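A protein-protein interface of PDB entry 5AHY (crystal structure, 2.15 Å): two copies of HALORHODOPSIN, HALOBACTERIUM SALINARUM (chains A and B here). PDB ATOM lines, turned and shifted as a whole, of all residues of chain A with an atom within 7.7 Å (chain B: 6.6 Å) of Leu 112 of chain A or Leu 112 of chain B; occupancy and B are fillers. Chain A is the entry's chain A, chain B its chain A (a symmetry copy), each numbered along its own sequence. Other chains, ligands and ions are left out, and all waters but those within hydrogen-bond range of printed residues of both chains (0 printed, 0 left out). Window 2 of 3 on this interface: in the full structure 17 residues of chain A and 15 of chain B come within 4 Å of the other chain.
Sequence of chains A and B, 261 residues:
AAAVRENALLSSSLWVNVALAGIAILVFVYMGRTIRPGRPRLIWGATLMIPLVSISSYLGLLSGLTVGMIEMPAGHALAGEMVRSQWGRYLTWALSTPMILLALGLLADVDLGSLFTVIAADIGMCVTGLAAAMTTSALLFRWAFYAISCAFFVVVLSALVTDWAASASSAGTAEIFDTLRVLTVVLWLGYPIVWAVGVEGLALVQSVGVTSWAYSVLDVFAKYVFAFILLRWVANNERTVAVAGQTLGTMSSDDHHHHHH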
ATOM      1  N   LEU A  42      31.190  17.056  26.476  1.00  0.00           N
ATOM      2  CA  LEU A  42      29.841  16.498  26.525  1.00  0.00           C
ATOM      3  C   LEU A  42      29.899  14.971  26.539  1.00  0.00           C
ATOM      4  O   LEU A  42      29.149  14.306  27.261  1.00  0.00           O
ATOM      5  CB  LEU A  42      29.013  16.981  25.326  1.00  0.00           C
ATOM      6  CG  LEU A  42      28.711  18.484  25.209  1.00  0.00           C
ATOM      7  CD1 LEU A  42      27.994  18.787  23.910  1.00  0.00           C
ATOM      8  CD2 LEU A  42      27.883  18.984  26.380  1.00  0.00           C
ATOM      9  N   LEU A 102      24.185   7.168  24.547  1.00  0.00           N
ATOM     10  CA  LEU A 102      24.327   8.616  24.460  1.00  0.00           C
ATOM     11  C   LEU A 102      25.784   9.021  24.176  1.00  0.00           C
ATOM     12  O   LEU A 102      26.039   9.934  23.403  1.00  0.00           O
ATOM     13  CB  LEU A 102      23.839   9.289  25.748  1.00  0.00           C
ATOM     14  CG  LEU A 102      24.016  10.815  25.824  1.00  0.00           C
ATOM     15  CD1 LEU A 102      23.375  11.532  24.624  1.00  0.00           C
ATOM     16  CD2 LEU A 102      23.448  11.346  27.134  1.00  0.00           C
ATOM     17  N   GLY A 105      26.345   8.270  20.670  1.00  0.00           N
ATOM     18  CA  GLY A 105      25.557   9.160  19.835  1.00  0.00           C
ATOM     19  C   GLY A 105      26.226  10.510  19.669  1.00  0.00           C
ATOM     20  O   GLY A 105      26.231  11.084  18.589  1.00  0.00           O
ATOM     21  N   LEU A 106      26.777  11.022  20.761  1.00  0.00           N
ATOM     22  CA  LEU A 106      27.545  12.252  20.739  1.00  0.00           C
ATOM     23  C   LEU A 106      28.788  12.088  19.875  1.00  0.00           C
ATOM     24  O   LEU A 106      29.130  12.973  19.088  1.00  0.00           O
ATOM     25  CB  LEU A 106      27.927  12.653  22.168  1.00  0.00           C
ATOM     26  CG  LEU A 106      26.713  13.081  22.989  1.00  0.00           C
ATOM     27  CD1 LEU A 106      27.067  13.320  24.461  1.00  0.00           C
ATOM     28  CD2 LEU A 106      26.109  14.340  22.348  1.00  0.00           C
ATOM     29  N   ASP A 109      27.760  11.903  16.250  1.00  0.00           N
ATOM     30  CA  ASP A 109      26.905  13.033  15.877  1.00  0.00           C
ATOM     31  C   ASP A 109      25.635  12.592  15.131  1.00  0.00           C
ATOM     32  O   ASP A 109      25.375  13.019  14.007  1.00  0.00           O
ATOM     33  CB  ASP A 109      27.696  14.032  15.027  1.00  0.00           C
ATOM     34  CG  ASP A 109      27.008  15.374  14.922  1.00  0.00           C
ATOM     35  OD1 ASP A 109      26.373  15.796  15.920  1.00  0.00           O
ATOM     36  OD2 ASP A 109      27.089  15.998  13.840  1.00  0.00           O
ATOM     37  N   VAL A 110      24.851  11.730  15.766  1.00  0.00           N
ATOM     38  CA  VAL A 110      23.701  11.129  15.120  1.00  0.00           C
ATOM     39  C   VAL A 110      22.504  12.074  15.072  1.00  0.00           C
ATOM     40  O   VAL A 110      22.453  13.066  15.790  1.00  0.00           O
ATOM     41  CB  VAL A 110      23.291   9.836  15.842  1.00  0.00           C
ATOM     42  CG1 VAL A 110      24.397   8.801  15.729  1.00  0.00           C
ATOM     43  CG2 VAL A 110      22.948  10.131  17.302  1.00  0.00           C
ATOM     44  N   ASP A 111      21.532  11.751  14.228  1.00  0.00           N
ATOM     45  CA  ASP A 111      20.258  12.457  14.240  1.00  0.00           C
ATOM     46  C   ASP A 111      19.540  12.212  15.555  1.00  0.00           C
ATOM     47  O   ASP A 111      19.455  11.068  16.017  1.00  0.00           O
ATOM     48  CB  ASP A 111      19.379  12.005  13.081  1.00  0.00           C
ATOM     49  CG  ASP A 111      20.019  12.260  11.733  1.00  0.00           C
ATOM     50  OD1 ASP A 111      20.821  13.217  11.628  1.00  0.00           O
ATOM     51  OD2 ASP A 111      19.718  11.503  10.782  1.00  0.00           O
ATOM     52  N   LEU A 112      19.017  13.282  16.145  1.00  0.00           N
ATOM     53  CA  LEU A 112      18.302  13.194  17.407  1.00  0.00           C
ATOM     54  C   LEU A 112      17.090  12.261  17.345  1.00  0.00           C
ATOM     55  O   LEU A 112      16.721  11.640  18.345  1.00  0.00           O
ATOM     56  CB  LEU A 112      17.867  14.581  17.845  1.00  0.00           C
ATOM     57  CG  LEU A 112      19.045  15.407  18.345  1.00  0.00           C
ATOM     58  CD1 LEU A 112      18.572  16.787  18.678  1.00  0.00           C
ATOM     59  CD2 LEU A 112      19.676  14.751  19.562  1.00  0.00           C
ATOM     60  N   GLY A 113      16.478  12.163  16.173  1.00  0.00           N
ATOM     61  CA  GLY A 113      15.348  11.282  15.996  1.00  0.00           C
ATOM     62  C   GLY A 113      15.803   9.843  16.125  1.00  0.00           C
ATOM     63  O   GLY A 113      15.120   9.028  16.734  1.00  0.00           O
ATOM     64  N   SER A 114      16.956   9.535  15.541  1.00  0.00           N
ATOM     65  CA  SER A 114      17.546   8.208  15.647  1.00  0.00           C
ATOM     66  C   SER A 114      17.909   7.906  17.108  1.00  0.00           C
ATOM     67  O   SER A 114      17.569   6.843  17.622  1.00  0.00           O
ATOM     68  CB  SER A 114      18.780   8.092  14.739  1.00  0.00           C
ATOM     69  OG  SER A 114      19.417   6.826  14.875  1.00  0.00           O
ATOM     70  N   LEU A 115      18.566   8.861  17.769  1.00  0.00           N
ATOM     71  CA  LEU A 115      18.913   8.751  19.185  1.00  0.00           C
ATOM     72  C   LEU A 115      17.724   8.394  20.079  1.00  0.00           C
ATOM     73  O   LEU A 115      17.824   7.500  20.919  1.00  0.00           O
ATOM     74  CB  LEU A 115      19.540  10.063  19.680  1.00  0.00           C
ATOM     75  CG  LEU A 115      19.876  10.131  21.173  1.00  0.00           C
ATOM     76  CD1 LEU A 115      21.135   9.309  21.494  1.00  0.00           C
ATOM     77  CD2 LEU A 115      20.005  11.579  21.667  1.00  0.00           C
ATOM     78  N   PHE A 116      16.606   9.091  19.899  1.00  0.00           N
ATOM     79  CA  PHE A 116      15.419   8.879  20.729  1.00  0.00           C
ATOM     80  C   PHE A 116      14.787   7.509  20.482  1.00  0.00           C
ATOM     81  O   PHE A 116      14.279   6.855  21.404  1.00  0.00           O
ATOM     82  CB  PHE A 116      14.367   9.970  20.471  1.00  0.00           C
ATOM     83  CG  PHE A 116      14.839  11.370  20.763  1.00  0.00           C
ATOM     84  CD1 PHE A 116      15.866  11.605  21.663  1.00  0.00           C
ATOM     85  CD2 PHE A 116      14.241  12.461  20.131  1.00  0.00           C
ATOM     86  CE1 PHE A 116      16.299  12.901  21.929  1.00  0.00           C
ATOM     87  CE2 PHE A 116      14.661  13.756  20.390  1.00  0.00           C
ATOM     88  CZ  PHE A 116      15.695  13.978  21.292  1.00  0.00           C
ATOM     89  N   THR A 117      14.795   7.083  19.228  1.00  0.00           N
ATOM     90  CA  THR A 117      14.236   5.776  18.888  1.00  0.00           C
ATOM     91  C   THR A 117      15.112   4.659  19.447  1.00  0.00           C
ATOM     92  O   THR A 117      14.612   3.688  20.022  1.00  0.00           O
ATOM     93  CB  THR A 117      14.092   5.605  17.368  1.00  0.00           C
ATOM     94  OG1 THR A 117      13.191   6.598  16.863  1.00  0.00           O
ATOM     95  CG2 THR A 117      13.558   4.203  17.028  1.00  0.00           C
ATOM     96  N   VAL A 118      16.426   4.802  19.282  1.00  0.00           N
ATOM     97  CA  VAL A 118      17.365   3.802  19.791  1.00  0.00           C
ATOM     98  C   VAL A 118      17.268   3.682  21.306  1.00  0.00           C
ATOM     99  O   VAL A 118      17.177   2.577  21.843  1.00  0.00           O
ATOM    100  CB  VAL A 118      18.820   4.135  19.401  1.00  0.00           C
ATOM    101  CG1 VAL A 118      19.789   3.172  20.069  1.00  0.00           C
ATOM    102  CG2 VAL A 118      18.980   4.085  17.887  1.00  0.00           C
ATOM    103  N   TRP A 164      24.091   5.122  12.406  1.00  0.00           N
ATOM    104  CA  TRP A 164      25.043   5.728  13.329  1.00  0.00           C
ATOM    105  C   TRP A 164      26.449   5.688  12.735  1.00  0.00           C
ATOM    106  O   TRP A 164      27.226   6.630  12.894  1.00  0.00           O
ATOM    107  CB  TRP A 164      24.992   5.031  14.692  1.00  0.00           C
ATOM    108  CG  TRP A 164      23.757   5.390  15.477  1.00  0.00           C
ATOM    109  CD1 TRP A 164      22.502   5.621  14.978  1.00  0.00           C
ATOM    110  CD2 TRP A 164      23.672   5.604  16.891  1.00  0.00           C
ATOM    111  NE1 TRP A 164      21.640   5.947  15.999  1.00  0.00           N
ATOM    112  CE2 TRP A 164      22.333   5.942  17.184  1.00  0.00           C
ATOM    113  CE3 TRP A 164      24.596   5.525  17.942  1.00  0.00           C
ATOM    114  CZ2 TRP A 164      21.895   6.204  18.486  1.00  0.00           C
ATOM    115  CZ3 TRP A 164      24.168   5.793  19.223  1.00  0.00           C
ATOM    116  CH2 TRP A 164      22.827   6.125  19.489  1.00  0.00           C
ATOM    117  N   VAL B 110      20.829  25.761  26.393  1.00  0.00           N
ATOM    118  CA  VAL B 110      21.978  24.897  26.574  1.00  0.00           C
ATOM    119  C   VAL B 110      22.141  23.901  25.428  1.00  0.00           C
ATOM    120  O   VAL B 110      21.217  23.671  24.656  1.00  0.00           O
ATOM    121  CB  VAL B 110      21.870  24.123  27.897  1.00  0.00           C
ATOM    122  CG1 VAL B 110      21.908  25.087  29.071  1.00  0.00           C
ATOM    123  CG2 VAL B 110      20.597  23.275  27.911  1.00  0.00           C
ATOM    124  N   ASP B 111      23.321  23.303  25.331  1.00  0.00           N
ATOM    125  CA  ASP B 111      23.530  22.192  24.411  1.00  0.00           C
ATOM    126  C   ASP B 111      22.679  21.006  24.827  1.00  0.00           C
ATOM    127  O   ASP B 111      22.645  20.644  26.010  1.00  0.00           O
ATOM    128  CB  ASP B 111      24.998  21.787  24.377  1.00  0.00           C
ATOM    129  CG  ASP B 111      25.901  22.916  23.928  1.00  0.00           C
ATOM    130  OD1 ASP B 111      25.430  23.781  23.154  1.00  0.00           O
ATOM    131  OD2 ASP B 111      27.080  22.934  24.348  1.00  0.00           O
ATOM    132  N   LEU B 112      22.007  20.397  23.855  1.00  0.00           N
ATOM    133  CA  LEU B 112      21.154  19.249  24.110  1.00  0.00           C
ATOM    134  C   LEU B 112      21.906  18.072  24.738  1.00  0.00           C
ATOM    135  O   LEU B 112      21.332  17.292  25.502  1.00  0.00           O
ATOM    136  CB  LEU B 112      20.490  18.809  22.817  1.00  0.00           C
ATOM    137  CG  LEU B 112      19.393  19.776  22.393  1.00  0.00           C
ATOM    138  CD1 LEU B 112      18.837  19.341  21.072  1.00  0.00           C
ATOM    139  CD2 LEU B 112      18.296  19.828  23.442  1.00  0.00           C
ATOM    140  N   GLY B 113      23.187  17.950  24.417  1.00  0.00           N
ATOM    141  CA  GLY B 113      23.997  16.899  24.985  1.00  0.00           C
ATOM    142  C   GLY B 113      24.166  17.134  26.470  1.00  0.00           C
ATOM    143  O   GLY B 113      24.105  16.198  27.259  1.00  0.00           O
ATOM    144  N   SER B 114      24.386  18.390  26.847  1.00  0.00           N
ATOM    145  CA  SER B 114      24.496  18.768  28.249  1.00  0.00           C
ATOM    146  C   SER B 114      23.164  18.514  28.970  1.00  0.00           C
ATOM    147  O   SER B 114      23.146  17.906  30.038  1.00  0.00           O
ATOM    148  CB  SER B 114      24.918  20.239  28.380  1.00  0.00           C
ATOM    149  OG  SER B 114      24.966  20.656  29.740  1.00  0.00           O
ATOM    150  N   LEU B 115      22.062  18.952  28.360  1.00  0.00           N
ATOM    151  CA  LEU B 115      20.717  18.717  28.884  1.00  0.00           C
ATOM    152  C   LEU B 115      20.435  17.250  29.209  1.00  0.00           C
ATOM    153  O   LEU B 115      19.928  16.936  30.285  1.00  0.00           O
ATOM    154  CB  LEU B 115      19.664  19.225  27.889  1.00  0.00           C
ATOM    155  CG  LEU B 115      18.201  18.967  28.261  1.00  0.00           C
ATOM    156  CD1 LEU B 115      17.736  19.925  29.371  1.00  0.00           C
ATOM    157  CD2 LEU B 115      17.276  19.031  27.037  1.00  0.00           C
ATOM    158  N   PHE B 116      20.764  16.355  28.281  1.00  0.00           N
ATOM    159  CA  PHE B 116      20.495  14.926  28.452  1.00  0.00           C
ATOM    160  C   PHE B 116      21.348  14.314  29.563  1.00  0.00           C
ATOM    161  O   PHE B 116      20.900  13.433  30.312  1.00  0.00           O
ATOM    162  CB  PHE B 116      20.751  14.159  27.144  1.00  0.00           C
ATOM    163  CG  PHE B 116      19.904  14.612  25.983  1.00  0.00           C
ATOM    164  CD1 PHE B 116      18.681  15.231  26.188  1.00  0.00           C
ATOM    165  CD2 PHE B 116      20.337  14.404  24.674  1.00  0.00           C
ATOM    166  CE1 PHE B 116      17.904  15.647  25.112  1.00  0.00           C
ATOM    167  CE2 PHE B 116      19.570  14.811  23.594  1.00  0.00           C
ATOM    168  CZ  PHE B 116      18.348  15.435  23.812  1.00  0.00           C
ATOM    169  N   THR B 117      22.590  14.762  29.658  1.00  0.00           N
ATOM    170  CA  THR B 117      23.480  14.260  30.701  1.00  0.00           C
ATOM    171  C   THR B 117      23.025  14.747  32.073  1.00  0.00           C
ATOM    172  O   THR B 117      22.980  13.976  33.037  1.00  0.00           O
ATOM    173  CB  THR B 117      24.934  14.694  30.457  1.00  0.00           C
ATOM    174  OG1 THR B 117      25.387  14.151  29.211  1.00  0.00           O
ATOM    175  CG2 THR B 117      25.845  14.204  31.596  1.00  0.00           C
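O of Gly 113 of chain B lies within hydrogen-bond range of OG1 of Thr 117 of chain B (3.1 Å).
Among the printed residues, merely in contact across the chains: Leu 42 of chain A with Ser 114 of chain B (3.6 Å), Leu 102 of chain A with Phe 116 of chain B (3.9 Å), Leu 102 of chain A with Thr 117 of chain B (3.99 Å), Leu 112 of chain A with Leu 112 of chain B (3.5 Å), Leu 115 of chain A with Phe 116 of chain B (3.8 Å) and Phe 116 of chain A with Phe 116 of chain B (3.8 Å).
Leu 112 of chain A touches just one residue of chain B: Leu 112 (3.5 Å). Of chain A, only Leu 112 (3.5 Å) comes within 4 Å of Leu 112 of chain B. Of the printed residues of chain B, Leu 115 of chain A touches Phe 116. Printed residues of chain B within 4 Å of Leu 42 of chain A: Ser 114 (3.6 Å). Of the printed residues of chain A, Thr 117 of chain B touches Leu 102 (3.99 Å). Printed residues of chain A within 4 Å of Phe 116 of chain B: Leu 102 (3.9 Å), Leu 115 (3.8 Å) and Phe 116 (3.8 Å). Val 110 of chain A touches none of the printed residues of chain B.
Hydrophobic or aromatic side chains of chain A within 4 Å of the printed part of chain B: Leu 42, Leu 102, Leu 112, Leu 115 and Phe 116. Along chain A the printed residues that touch a printed residue of chain B span positions 42 to 116. Of the 8 printed residues of chain B, 4 touch a printed residue of chain A. Among the printed residues, 6 pairs touch across the chains.
Leu 112 of chain A touches its own counterpart, Leu 112 of chain B. Leu 115 of chain A touches Phe 116 of chain B, but with the chains exchanged Phe 116 of chain A does not touch Leu 115 of chain B (7.8 Å). Phe 116 of chain B touches its own counterpart, Phe 116 of chain A. Positions printed for both chains: 110, 111, 112, 113, 114, 115, 116 and 117.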
